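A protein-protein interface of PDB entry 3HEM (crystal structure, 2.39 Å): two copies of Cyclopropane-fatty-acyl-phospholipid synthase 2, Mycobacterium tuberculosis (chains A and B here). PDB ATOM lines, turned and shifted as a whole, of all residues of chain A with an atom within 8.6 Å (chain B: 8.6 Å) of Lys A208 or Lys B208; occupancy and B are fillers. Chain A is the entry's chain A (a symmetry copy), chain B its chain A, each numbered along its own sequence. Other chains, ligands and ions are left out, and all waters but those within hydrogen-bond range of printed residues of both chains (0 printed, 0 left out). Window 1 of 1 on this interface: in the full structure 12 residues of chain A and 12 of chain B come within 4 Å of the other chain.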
ATOM      1  N   MET A 201     -16.471  20.858  -0.307  1.00  0.00           N
ATOM      2  CA  MET A 201     -15.029  21.000  -0.129  1.00  0.00           C
ATOM      3  C   MET A 201     -14.410  19.699   0.376  1.00  0.00           C
ATOM      4  O   MET A 201     -13.296  19.325  -0.014  1.00  0.00           O
ATOM      5  CB  MET A 201     -14.705  22.154   0.818  1.00  0.00           C
ATOM      6  CG  MET A 201     -13.208  22.407   0.972  1.00  0.00           C
ATOM      7  SD  MET A 201     -12.489  23.286  -0.428  1.00  0.00           S
ATOM      8  CE  MET A 201     -10.862  22.544  -0.520  1.00  0.00           C
ATOM      9  N   SER A 202     -15.150  19.015   1.241  1.00  0.00           N
ATOM     10  CA  SER A 202     -14.721  17.727   1.772  1.00  0.00           C
ATOM     11  C   SER A 202     -14.381  16.760   0.652  1.00  0.00           C
ATOM     12  O   SER A 202     -13.353  16.082   0.697  1.00  0.00           O
ATOM     13  CB  SER A 202     -15.806  17.142   2.678  1.00  0.00           C
ATOM     14  OG  SER A 202     -17.081  17.697   2.373  1.00  0.00           O
ATOM     15  N   LEU A 203     -15.236  16.712  -0.365  1.00  0.00           N
ATOM     16  CA  LEU A 203     -15.005  15.836  -1.506  1.00  0.00           C
ATOM     17  C   LEU A 203     -13.733  16.213  -2.268  1.00  0.00           C
ATOM     18  O   LEU A 203     -12.905  15.354  -2.595  1.00  0.00           O
ATOM     19  CB  LEU A 203     -16.210  15.847  -2.439  1.00  0.00           C
ATOM     20  CG  LEU A 203     -15.936  15.256  -3.819  1.00  0.00           C
ATOM     21  CD1 LEU A 203     -15.193  13.953  -3.706  1.00  0.00           C
ATOM     22  CD2 LEU A 203     -17.240  15.037  -4.523  1.00  0.00           C
ATOM     23  N   LEU A 204     -13.585  17.502  -2.552  1.00  0.00           N
ATOM     24  CA  LEU A 204     -12.401  17.996  -3.237  1.00  0.00           C
ATOM     25  C   LEU A 204     -11.119  17.658  -2.464  1.00  0.00           C
ATOM     26  O   LEU A 204     -10.123  17.228  -3.055  1.00  0.00           O
ATOM     27  CB  LEU A 204     -12.526  19.501  -3.494  1.00  0.00           C
ATOM     28  CG  LEU A 204     -13.721  19.908  -4.371  1.00  0.00           C
ATOM     29  CD1 LEU A 204     -13.921  21.399  -4.345  1.00  0.00           C
ATOM     30  CD2 LEU A 204     -13.560  19.436  -5.804  1.00  0.00           C
ATOM     31  N   ARG A 205     -11.154  17.831  -1.142  1.00  0.00           N
ATOM     32  CA  ARG A 205     -10.032  17.438  -0.297  1.00  0.00           C
ATOM     33  C   ARG A 205      -9.742  15.946  -0.445  1.00  0.00           C
ATOM     34  O   ARG A 205      -8.582  15.516  -0.439  1.00  0.00           O
ATOM     35  CB  ARG A 205     -10.314  17.776   1.169  1.00  0.00           C
ATOM     36  CG  ARG A 205     -10.076  19.235   1.542  1.00  0.00           C
ATOM     37  CD  ARG A 205     -10.473  19.527   3.000  1.00  0.00           C
ATOM     38  NE  ARG A 205      -9.989  18.514   3.940  1.00  0.00           N
ATOM     39  CZ  ARG A 205      -8.717  18.390   4.325  1.00  0.00           C
ATOM     40  NH1 ARG A 205      -7.779  19.220   3.856  1.00  0.00           N
ATOM     41  NH2 ARG A 205      -8.376  17.427   5.181  1.00  0.00           N
ATOM     42  N   PHE A 206     -10.803  15.158  -0.591  1.00  0.00           N
ATOM     43  CA  PHE A 206     -10.646  13.716  -0.652  1.00  0.00           C
ATOM     44  C   PHE A 206      -9.976  13.261  -1.939  1.00  0.00           C
ATOM     45  O   PHE A 206      -9.037  12.456  -1.924  1.00  0.00           O
ATOM     46  CB  PHE A 206     -11.976  12.998  -0.485  1.00  0.00           C
ATOM     47  CG  PHE A 206     -11.824  11.516  -0.314  1.00  0.00           C
ATOM     48  CD1 PHE A 206     -11.235  10.998   0.828  1.00  0.00           C
ATOM     49  CD2 PHE A 206     -12.252  10.640  -1.300  1.00  0.00           C
ATOM     50  CE1 PHE A 206     -11.083   9.641   0.983  1.00  0.00           C
ATOM     51  CE2 PHE A 206     -12.105   9.279  -1.145  1.00  0.00           C
ATOM     52  CZ  PHE A 206     -11.520   8.780  -0.005  1.00  0.00           C
ATOM     53  N   ILE A 207     -10.477  13.757  -3.059  1.00  0.00           N
ATOM     54  CA  ILE A 207      -9.894  13.398  -4.330  1.00  0.00           C
ATOM     55  C   ILE A 207      -8.422  13.751  -4.297  1.00  0.00           C
ATOM     56  O   ILE A 207      -7.564  12.955  -4.678  1.00  0.00           O
ATOM     57  CB  ILE A 207     -10.548  14.149  -5.467  1.00  0.00           C
ATOM     58  CG1 ILE A 207     -12.014  13.732  -5.582  1.00  0.00           C
ATOM     59  CG2 ILE A 207      -9.771  13.921  -6.750  1.00  0.00           C
ATOM     60  CD1 ILE A 207     -12.212  12.253  -5.717  1.00  0.00           C
ATOM     61  N   LYS A 208      -8.131  14.956  -3.829  1.00  0.00           N
ATOM     62  CA  LYS A 208      -6.755  15.383  -3.712  1.00  0.00           C
ATOM     63  C   LYS A 208      -5.995  14.334  -2.903  1.00  0.00           C
ATOM     64  O   LYS A 208      -4.934  13.868  -3.313  1.00  0.00           O
ATOM     65  CB  LYS A 208      -6.688  16.757  -3.054  1.00  0.00           C
ATOM     66  CG  LYS A 208      -5.281  17.284  -2.856  1.00  0.00           C
ATOM     67  CD  LYS A 208      -4.711  16.873  -1.508  1.00  0.00           C
ATOM     68  CE  LYS A 208      -3.245  17.247  -1.437  1.00  0.00           C
ATOM     69  NZ  LYS A 208      -2.564  16.667  -0.255  1.00  0.00           N
ATOM     70  N   PHE A 209      -6.555  13.940  -1.767  1.00  0.00           N
ATOM     71  CA  PHE A 209      -5.925  12.917  -0.943  1.00  0.00           C
ATOM     72  C   PHE A 209      -5.710  11.631  -1.740  1.00  0.00           C
ATOM     73  O   PHE A 209      -4.657  10.996  -1.643  1.00  0.00           O
ATOM     74  CB  PHE A 209      -6.771  12.656   0.301  1.00  0.00           C
ATOM     75  CG  PHE A 209      -6.546  11.316   0.919  1.00  0.00           C
ATOM     76  CD1 PHE A 209      -5.461  11.088   1.740  1.00  0.00           C
ATOM     77  CD2 PHE A 209      -7.436  10.282   0.698  1.00  0.00           C
ATOM     78  CE1 PHE A 209      -5.267   9.844   2.321  1.00  0.00           C
ATOM     79  CE2 PHE A 209      -7.242   9.045   1.267  1.00  0.00           C
ATOM     80  CZ  PHE A 209      -6.162   8.825   2.075  1.00  0.00           C
ATOM     81  N   ILE A 210      -6.704  11.255  -2.539  1.00  0.00           N
ATOM     82  CA  ILE A 210      -6.597  10.046  -3.340  1.00  0.00           C
ATOM     83  C   ILE A 210      -5.489  10.152  -4.367  1.00  0.00           C
ATOM     84  O   ILE A 210      -4.649   9.262  -4.478  1.00  0.00           O
ATOM     85  CB  ILE A 210      -7.891   9.732  -4.078  1.00  0.00           C
ATOM     86  CG1 ILE A 210      -9.007   9.425  -3.088  1.00  0.00           C
ATOM     87  CG2 ILE A 210      -7.680   8.539  -4.983  1.00  0.00           C
ATOM     88  CD1 ILE A 210      -8.684   8.272  -2.154  1.00  0.00           C
ATOM     89  N   LEU A 211      -5.493  11.242  -5.124  1.00  0.00           N
ATOM     90  CA  LEU A 211      -4.512  11.427  -6.181  1.00  0.00           C
ATOM     91  C   LEU A 211      -3.151  11.726  -5.605  1.00  0.00           C
ATOM     92  O   LEU A 211      -2.153  11.729  -6.316  1.00  0.00           O
ATOM     93  CB  LEU A 211      -4.930  12.561  -7.099  1.00  0.00           C
ATOM     94  CG  LEU A 211      -6.072  12.173  -8.033  1.00  0.00           C
ATOM     95  CD1 LEU A 211      -6.597  13.389  -8.774  1.00  0.00           C
ATOM     96  CD2 LEU A 211      -5.612  11.086  -8.999  1.00  0.00           C
ATOM     97  N   THR A 212      -3.112  11.973  -4.306  1.00  0.00           N
ATOM     98  CA  THR A 212      -1.859  12.289  -3.655  1.00  0.00           C
ATOM     99  C   THR A 212      -1.288  11.068  -2.962  1.00  0.00           C
ATOM    100  O   THR A 212      -0.145  10.712  -3.194  1.00  0.00           O
ATOM    101  CB  THR A 212      -2.026  13.411  -2.628  1.00  0.00           C
ATOM    102  OG1 THR A 212      -2.570  14.569  -3.271  1.00  0.00           O
ATOM    103  CG2 THR A 212      -0.684  13.760  -2.015  1.00  0.00           C
ATOM    104  N   GLU A 213      -2.089  10.412  -2.127  1.00  0.00           N
ATOM    105  CA  GLU A 213      -1.578   9.325  -1.303  1.00  0.00           C
ATOM    106  C   GLU A 213      -1.838   7.929  -1.862  1.00  0.00           C
ATOM    107  O   GLU A 213      -1.185   6.971  -1.453  1.00  0.00           O
ATOM    108  CB  GLU A 213      -2.174   9.412   0.096  1.00  0.00           C
ATOM    109  CG  GLU A 213      -1.958  10.753   0.750  1.00  0.00           C
ATOM    110  CD  GLU A 213      -0.536  10.935   1.224  1.00  0.00           C
ATOM    111  OE1 GLU A 213       0.138   9.907   1.448  1.00  0.00           O
ATOM    112  OE2 GLU A 213      -0.104  12.101   1.378  1.00  0.00           O
ATOM    113  N   ILE A 214      -2.793   7.795  -2.774  1.00  0.00           N
ATOM    114  CA  ILE A 214      -3.182   6.462  -3.215  1.00  0.00           C
ATOM    115  C   ILE A 214      -2.861   6.181  -4.678  1.00  0.00           C
ATOM    116  O   ILE A 214      -2.000   5.354  -4.970  1.00  0.00           O
ATOM    117  CB  ILE A 214      -4.662   6.192  -2.942  1.00  0.00           C
ATOM    118  CG1 ILE A 214      -5.037   6.669  -1.540  1.00  0.00           C
ATOM    119  CG2 ILE A 214      -4.946   4.714  -3.066  1.00  0.00           C
ATOM    120  CD1 ILE A 214      -4.267   6.000  -0.434  1.00  0.00           C
ATOM    121  N   PHE A 215      -3.531   6.877  -5.593  1.00  0.00           N
ATOM    122  CA  PHE A 215      -3.376   6.595  -7.019  1.00  0.00           C
ATOM    123  C   PHE A 215      -2.888   7.786  -7.824  1.00  0.00           C
ATOM    124  O   PHE A 215      -3.640   8.378  -8.600  1.00  0.00           O
ATOM    125  CB  PHE A 215      -4.688   6.084  -7.609  1.00  0.00           C
ATOM    126  CG  PHE A 215      -5.182   4.819  -6.976  1.00  0.00           C
ATOM    127  CD1 PHE A 215      -6.349   4.814  -6.231  1.00  0.00           C
ATOM    128  CD2 PHE A 215      -4.474   3.633  -7.124  1.00  0.00           C
ATOM    129  CE1 PHE A 215      -6.807   3.648  -5.645  1.00  0.00           C
ATOM    130  CE2 PHE A 215      -4.925   2.454  -6.541  1.00  0.00           C
ATOM    131  CZ  PHE A 215      -6.096   2.461  -5.801  1.00  0.00           C
ATOM    132  N   PRO A 216      -1.608   8.120  -7.663  1.00  0.00           N
ATOM    133  CA  PRO A 216      -0.965   9.216  -8.385  1.00  0.00           C
ATOM    134  C   PRO A 216      -1.152   9.080  -9.889  1.00  0.00           C
ATOM    135  O   PRO A 216      -0.839   8.030 -10.453  1.00  0.00           O
ATOM    136  CB  PRO A 216       0.510   9.027  -8.030  1.00  0.00           C
ATOM    137  CG  PRO A 216       0.485   8.389  -6.692  1.00  0.00           C
ATOM    138  CD  PRO A 216      -0.668   7.436  -6.760  1.00  0.00           C
ATOM    139  N   GLY A 217      -1.650  10.128 -10.535  1.00  0.00           N
ATOM    140  CA  GLY A 217      -1.744  10.136 -11.984  1.00  0.00           C
ATOM    141  C   GLY A 217      -2.936   9.383 -12.545  1.00  0.00           C
ATOM    142  O   GLY A 217      -3.174   9.408 -13.755  1.00  0.00           O
ATOM    143  N   HIS A 279      -8.921   5.502   5.764  1.00  0.00           N
ATOM    144  CA  HIS A 279      -9.471   6.733   5.207  1.00  0.00           C
ATOM    145  C   HIS A 279      -9.792   6.569   3.722  1.00  0.00           C
ATOM    146  O   HIS A 279     -10.892   6.888   3.278  1.00  0.00           O
ATOM    147  CB  HIS A 279      -8.517   7.918   5.448  1.00  0.00           C
ATOM    148  CG  HIS A 279      -9.050   9.232   4.963  1.00  0.00           C
ATOM    149  ND1 HIS A 279     -10.239   9.763   5.411  1.00  0.00           N
ATOM    150  CD2 HIS A 279      -8.557  10.117   4.062  1.00  0.00           C
ATOM    151  CE1 HIS A 279     -10.459  10.918   4.805  1.00  0.00           C
ATOM    152  NE2 HIS A 279      -9.454  11.155   3.981  1.00  0.00           N
ATOM    153  N   MET B 201     -12.514  15.442 -15.100  1.00  0.00           N
ATOM    154  CA  MET B 201     -11.319  14.929 -14.437  1.00  0.00           C
ATOM    155  C   MET B 201     -10.221  15.988 -14.392  1.00  0.00           C
ATOM    156  O   MET B 201      -9.476  16.100 -13.410  1.00  0.00           O
ATOM    157  CB  MET B 201     -10.817  13.658 -15.118  1.00  0.00           C
ATOM    158  CG  MET B 201      -9.619  13.026 -14.414  1.00  0.00           C
ATOM    159  SD  MET B 201     -10.074  12.110 -12.929  1.00  0.00           S
ATOM    160  CE  MET B 201      -8.666  12.424 -11.868  1.00  0.00           C
ATOM    161  N   SER B 202     -10.136  16.765 -15.467  1.00  0.00           N
ATOM    162  CA  SER B 202      -9.175  17.856 -15.555  1.00  0.00           C
ATOM    163  C   SER B 202      -9.303  18.793 -14.367  1.00  0.00           C
ATOM    164  O   SER B 202      -8.301  19.185 -13.765  1.00  0.00           O
ATOM    165  CB  SER B 202      -9.362  18.621 -16.867  1.00  0.00           C
ATOM    166  OG  SER B 202     -10.673  18.430 -17.386  1.00  0.00           O
ATOM    167  N   LEU B 203     -10.539  19.136 -14.017  1.00  0.00           N
ATOM    168  CA  LEU B 203     -10.787  20.015 -12.881  1.00  0.00           C
ATOM    169  C   LEU B 203     -10.320  19.393 -11.564  1.00  0.00           C
ATOM    170  O   LEU B 203      -9.641  20.039 -10.758  1.00  0.00           O
ATOM    171  CB  LEU B 203     -12.264  20.381 -12.804  1.00  0.00           C
ATOM    172  CG  LEU B 203     -12.686  20.993 -11.472  1.00  0.00           C
ATOM    173  CD1 LEU B 203     -11.713  22.054 -11.037  1.00  0.00           C
ATOM    174  CD2 LEU B 203     -14.053  21.588 -11.620  1.00  0.00           C
ATOM    175  N   LEU B 204     -10.688  18.135 -11.351  1.00  0.00           N
ATOM    176  CA  LEU B 204     -10.275  17.415 -10.155  1.00  0.00           C
ATOM    177  C   LEU B 204      -8.746  17.358 -10.033  1.00  0.00           C
ATOM    178  O   LEU B 204      -8.195  17.570  -8.947  1.00  0.00           O
ATOM    179  CB  LEU B 204     -10.897  16.016 -10.138  1.00  0.00           C
ATOM    180  CG  LEU B 204     -12.434  15.994 -10.131  1.00  0.00           C
ATOM    181  CD1 LEU B 204     -12.951  14.604 -10.386  1.00  0.00           C
ATOM    182  CD2 LEU B 204     -13.005  16.522  -8.830  1.00  0.00           C
ATOM    183  N   ARG B 205      -8.066  17.094 -11.148  1.00  0.00           N
ATOM    184  CA  ARG B 205      -6.607  17.123 -11.169  1.00  0.00           C
ATOM    185  C   ARG B 205      -6.089  18.502 -10.765  1.00  0.00           C
ATOM    186  O   ARG B 205      -5.069  18.625 -10.075  1.00  0.00           O
ATOM    187  CB  ARG B 205      -6.079  16.751 -12.557  1.00  0.00           C
ATOM    188  CG  ARG B 205      -6.047  15.254 -12.844  1.00  0.00           C
ATOM    189  CD  ARG B 205      -5.601  14.955 -14.287  1.00  0.00           C
ATOM    190  NE  ARG B 205      -4.433  15.735 -14.700  1.00  0.00           N
ATOM    191  CZ  ARG B 205      -3.187  15.505 -14.281  1.00  0.00           C
ATOM    192  NH1 ARG B 205      -2.928  14.506 -13.430  1.00  0.00           N
ATOM    193  NH2 ARG B 205      -2.191  16.279 -14.710  1.00  0.00           N
ATOM    194  N   PHE B 206      -6.806  19.540 -11.185  1.00  0.00           N
ATOM    195  CA  PHE B 206      -6.355  20.897 -10.931  1.00  0.00           C
ATOM    196  C   PHE B 206      -6.449  21.270  -9.460  1.00  0.00           C
ATOM    197  O   PHE B 206      -5.502  21.809  -8.874  1.00  0.00           O
ATOM    198  CB  PHE B 206      -7.122  21.909 -11.766  1.00  0.00           C
ATOM    199  CG  PHE B 206      -6.533  23.287 -11.701  1.00  0.00           C
ATOM    200  CD1 PHE B 206      -5.292  23.548 -12.259  1.00  0.00           C
ATOM    201  CD2 PHE B 206      -7.209  24.318 -11.069  1.00  0.00           C
ATOM    202  CE1 PHE B 206      -4.744  24.806 -12.191  1.00  0.00           C
ATOM    203  CE2 PHE B 206      -6.664  25.582 -11.002  1.00  0.00           C
ATOM    204  CZ  PHE B 206      -5.432  25.826 -11.562  1.00  0.00           C
ATOM    205  N   ILE B 207      -7.602  21.007  -8.868  1.00  0.00           N
ATOM    206  CA  ILE B 207      -7.779  21.309  -7.467  1.00  0.00           C
ATOM    207  C   ILE B 207      -6.696  20.596  -6.686  1.00  0.00           C
ATOM    208  O   ILE B 207      -6.042  21.179  -5.821  1.00  0.00           O
ATOM    209  CB  ILE B 207      -9.127  20.840  -6.969  1.00  0.00           C
ATOM    210  CG1 ILE B 207     -10.235  21.619  -7.675  1.00  0.00           C
ATOM    211  CG2 ILE B 207      -9.190  20.967  -5.459  1.00  0.00           C
ATOM    212  CD1 ILE B 207     -10.096  23.107  -7.558  1.00  0.00           C
ATOM    213  N   LYS B 208      -6.504  19.324  -6.999  1.00  0.00           N
ATOM    214  CA  LYS B 208      -5.468  18.557  -6.345  1.00  0.00           C
ATOM    215  C   LYS B 208      -4.149  19.313  -6.491  1.00  0.00           C
ATOM    216  O   LYS B 208      -3.435  19.529  -5.516  1.00  0.00           O
ATOM    217  CB  LYS B 208      -5.386  17.161  -6.956  1.00  0.00           C
ATOM    218  CG  LYS B 208      -4.304  16.284  -6.361  1.00  0.00           C
ATOM    219  CD  LYS B 208      -2.987  16.429  -7.107  1.00  0.00           C
ATOM    220  CE  LYS B 208      -1.893  15.695  -6.360  1.00  0.00           C
ATOM    221  NZ  LYS B 208      -0.542  15.989  -6.893  1.00  0.00           N
ATOM    222  N   PHE B 209      -3.842  19.742  -7.709  1.00  0.00           N
ATOM    223  CA  PHE B 209      -2.623  20.505  -7.943  1.00  0.00           C
ATOM    224  C   PHE B 209      -2.585  21.756  -7.065  1.00  0.00           C
ATOM    225  O   PHE B 209      -1.546  22.095  -6.494  1.00  0.00           O
ATOM    226  CB  PHE B 209      -2.512  20.869  -9.422  1.00  0.00           C
ATOM    227  CG  PHE B 209      -1.648  22.056  -9.692  1.00  0.00           C
ATOM    228  CD1 PHE B 209      -0.274  21.937  -9.728  1.00  0.00           C
ATOM    229  CD2 PHE B 209      -2.211  23.295  -9.934  1.00  0.00           C
ATOM    230  CE1 PHE B 209       0.521  23.042  -9.993  1.00  0.00           C
ATOM    231  CE2 PHE B 209      -1.425  24.394 -10.190  1.00  0.00           C
ATOM    232  CZ  PHE B 209      -0.064  24.270 -10.220  1.00  0.00           C
ATOM    233  N   ILE B 210      -3.723  22.432  -6.947  1.00  0.00           N
ATOM    234  CA  ILE B 210      -3.792  23.635  -6.134  1.00  0.00           C
ATOM    235  C   ILE B 210      -3.535  23.337  -4.671  1.00  0.00           C
ATOM    236  O   ILE B 210      -2.717  23.994  -4.030  1.00  0.00           O
ATOM    237  CB  ILE B 210      -5.147  24.322  -6.239  1.00  0.00           C
ATOM    238  CG1 ILE B 210      -5.380  24.819  -7.661  1.00  0.00           C
ATOM    239  CG2 ILE B 210      -5.197  25.492  -5.283  1.00  0.00           C
ATOM    240  CD1 ILE B 210      -4.306  25.776  -8.150  1.00  0.00           C
ATOM    241  N   LEU B 211      -4.243  22.348  -4.140  1.00  0.00           N
ATOM    242  CA  LEU B 211      -4.122  22.007  -2.732  1.00  0.00           C
ATOM    243  C   LEU B 211      -2.804  21.331  -2.454  1.00  0.00           C
ATOM    244  O   LEU B 211      -2.428  21.134  -1.304  1.00  0.00           O
ATOM    245  CB  LEU B 211      -5.257  21.091  -2.310  1.00  0.00           C
ATOM    246  CG  LEU B 211      -6.586  21.827  -2.163  1.00  0.00           C
ATOM    247  CD1 LEU B 211      -7.723  20.846  -1.953  1.00  0.00           C
ATOM    248  CD2 LEU B 211      -6.501  22.838  -1.025  1.00  0.00           C
ATOM    249  N   THR B 212      -2.096  20.979  -3.514  1.00  0.00           N
ATOM    250  CA  THR B 212      -0.824  20.306  -3.360  1.00  0.00           C
ATOM    251  C   THR B 212       0.324  21.286  -3.505  1.00  0.00           C
ATOM    252  O   THR B 212       1.177  21.360  -2.636  1.00  0.00           O
ATOM    253  CB  THR B 212      -0.652  19.184  -4.385  1.00  0.00           C
ATOM    254  OG1 THR B 212      -1.735  18.256  -4.260  1.00  0.00           O
ATOM    255  CG2 THR B 212       0.660  18.461  -4.151  1.00  0.00           C
ATOM    256  N   GLU B 213       0.336  22.053  -4.590  1.00  0.00           N
ATOM    257  CA  GLU B 213       1.479  22.907  -4.888  1.00  0.00           C
ATOM    258  C   GLU B 213       1.308  24.363  -4.466  1.00  0.00           C
ATOM    259  O   GLU B 213       2.292  25.091  -4.351  1.00  0.00           O
ATOM    260  CB  GLU B 213       1.786  22.861  -6.379  1.00  0.00           C
ATOM    261  CG  GLU B 213       1.991  21.460  -6.899  1.00  0.00           C
ATOM    262  CD  GLU B 213       3.328  20.890  -6.492  1.00  0.00           C
ATOM    263  OE1 GLU B 213       4.241  21.695  -6.208  1.00  0.00           O
ATOM    264  OE2 GLU B 213       3.461  19.644  -6.465  1.00  0.00           O
ATOM    265  N   ILE B 214       0.074  24.807  -4.251  1.00  0.00           N
ATOM    266  CA  ILE B 214      -0.147  26.224  -4.006  1.00  0.00           C
ATOM    267  C   ILE B 214      -0.657  26.532  -2.603  1.00  0.00           C
ATOM    268  O   ILE B 214       0.059  27.137  -1.808  1.00  0.00           O
ATOM    269  CB  ILE B 214      -1.082  26.835  -5.048  1.00  0.00           C
ATOM    270  CG1 ILE B 214      -0.698  26.357  -6.447  1.00  0.00           C
ATOM    271  CG2 ILE B 214      -1.004  28.342  -4.991  1.00  0.00           C
ATOM    272  CD1 ILE B 214       0.702  26.719  -6.862  1.00  0.00           C
ATOM    273  N   PHE B 215      -1.877  26.102  -2.292  1.00  0.00           N
ATOM    274  CA  PHE B 215      -2.496  26.450  -1.014  1.00  0.00           C
ATOM    275  C   PHE B 215      -2.871  25.243  -0.172  1.00  0.00           C
ATOM    276  O   PHE B 215      -4.050  24.922  -0.012  1.00  0.00           O
ATOM    277  CB  PHE B 215      -3.731  27.320  -1.235  1.00  0.00           C
ATOM    278  CG  PHE B 215      -3.440  28.613  -1.933  1.00  0.00           C
ATOM    279  CD1 PHE B 215      -3.929  28.852  -3.208  1.00  0.00           C
ATOM    280  CD2 PHE B 215      -2.672  29.592  -1.314  1.00  0.00           C
ATOM    281  CE1 PHE B 215      -3.662  30.044  -3.854  1.00  0.00           C
ATOM    282  CE2 PHE B 215      -2.397  30.795  -1.954  1.00  0.00           C
ATOM    283  CZ  PHE B 215      -2.894  31.023  -3.227  1.00  0.00           C
ATOM    284  N   PRO B 216      -1.861  24.586   0.398  1.00  0.00           N
ATOM    285  CA  PRO B 216      -2.043  23.425   1.267  1.00  0.00           C
ATOM    286  C   PRO B 216      -3.012  23.725   2.403  1.00  0.00           C
ATOM    287  O   PRO B 216      -2.824  24.704   3.126  1.00  0.00           O
ATOM    288  CB  PRO B 216      -0.638  23.209   1.831  1.00  0.00           C
ATOM    289  CG  PRO B 216       0.263  23.724   0.773  1.00  0.00           C
ATOM    290  CD  PRO B 216      -0.440  24.938   0.248  1.00  0.00           C
ATOM    291  N   GLY B 217      -4.032  22.890   2.563  1.00  0.00           N
ATOM    292  CA  GLY B 217      -4.932  23.022   3.695  1.00  0.00           C
ATOM    293  C   GLY B 217      -5.996  24.093   3.538  1.00  0.00           C
ATOM    294  O   GLY B 217      -6.876  24.225   4.389  1.00  0.00           O
ATOM    295  N   HIS B 279       0.708  27.872 -14.542  1.00  0.00           N
ATOM    296  CA  HIS B 279      -0.348  26.868 -14.499  1.00  0.00           C
ATOM    297  C   HIS B 279      -1.404  27.226 -13.452  1.00  0.00           C
ATOM    298  O   HIS B 279      -2.597  27.230 -13.741  1.00  0.00           O
ATOM    299  CB  HIS B 279       0.238  25.466 -14.247  1.00  0.00           C
ATOM    300  CG  HIS B 279      -0.785  24.371 -14.259  1.00  0.00           C
ATOM    301  ND1 HIS B 279      -1.594  24.121 -15.345  1.00  0.00           N
ATOM    302  CD2 HIS B 279      -1.134  23.465 -13.312  1.00  0.00           C
ATOM    303  CE1 HIS B 279      -2.401  23.111 -15.067  1.00  0.00           C
ATOM    304  NE2 HIS B 279      -2.142  22.696 -13.840  1.00  0.00           N
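Of the printed residues of chain B, Met A201 touches Leu B211.
Lys A208 touches just these residues of chain B: Lys B208, Leu B211 and Thr B212.
Of the printed residues of chain B, Leu A211 touches Met B201 (3.8 Å) and Lys B208 (3.8 Å).
Printed residues of chain B within 4 Å of Thr A212: Lys B208 (3.4 Å) and Thr B212 (3.9 Å).
Printed residues of chain A within 4 Å of Lys B208: Lys A208, Leu A211 and Thr A212.
Of the printed residues of chain A, Leu B211 touches Met A201 (3.8 Å) and Lys A208 (3.8 Å).
The nearest printed residue of chain A that does not touch Met B201 is Ile A207 (5.4 Å).
The side-chain hydroxyl (OG1) of Thr B212 sits at hydrogen-bond distance from the backbone carbonyl oxygen (O) of Lys B208.
The backbone carbonyl oxygen of Lys A208 is in hydrogen-bond range of the side-chain hydroxyl of Thr A212 (2.5 Å).
Lys A208 touches its own counterpart, Lys B208.
Lys A208 touches Leu B211, and with the chains exchanged Leu A211 touches Lys B208.
Lys A208 touches Thr B212, and with the chains exchanged Thr A212 touches Lys B208.
Thr A212 touches its own counterpart, Thr B212.
18 positions are printed for both chains.
Of the 8 pairs that touch across the chains among the printed residues, 8 have their exchanged pair printed and touching as well.
Among the printed residues, merely in contact across the chains: Lys A208 with Thr B212 (3.4 Å), Thr A212 with Lys B208 (3.4 Å), Lys A208 with Lys B208 (3.7 Å), Leu A211 with Met B201 (3.8 Å), Met A201 with Leu B211 (3.8 Å), Lys A208 with Leu B211 (3.8 Å), Leu A211 with Lys B208 (3.8 Å) and Thr A212 with Thr B212 (3.9 Å).
Along chain A the printed residues that touch a printed residue of chain B span positions 201 to 212.
Printed residues of chain B that touch a printed residue of chain A: Met B201, Lys B208, Leu B211 and Thr B212.
Hydrophobic or aromatic side chains of chain B that line the printed part of chain A: Met B201 and Leu B211.
Among the printed residues, 8 pairs touch across the chains.
Among the printed residues, no Asp or Glu carboxylate lies within 4 Å of a Lys or Arg side-chain nitrogen of the other chain.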
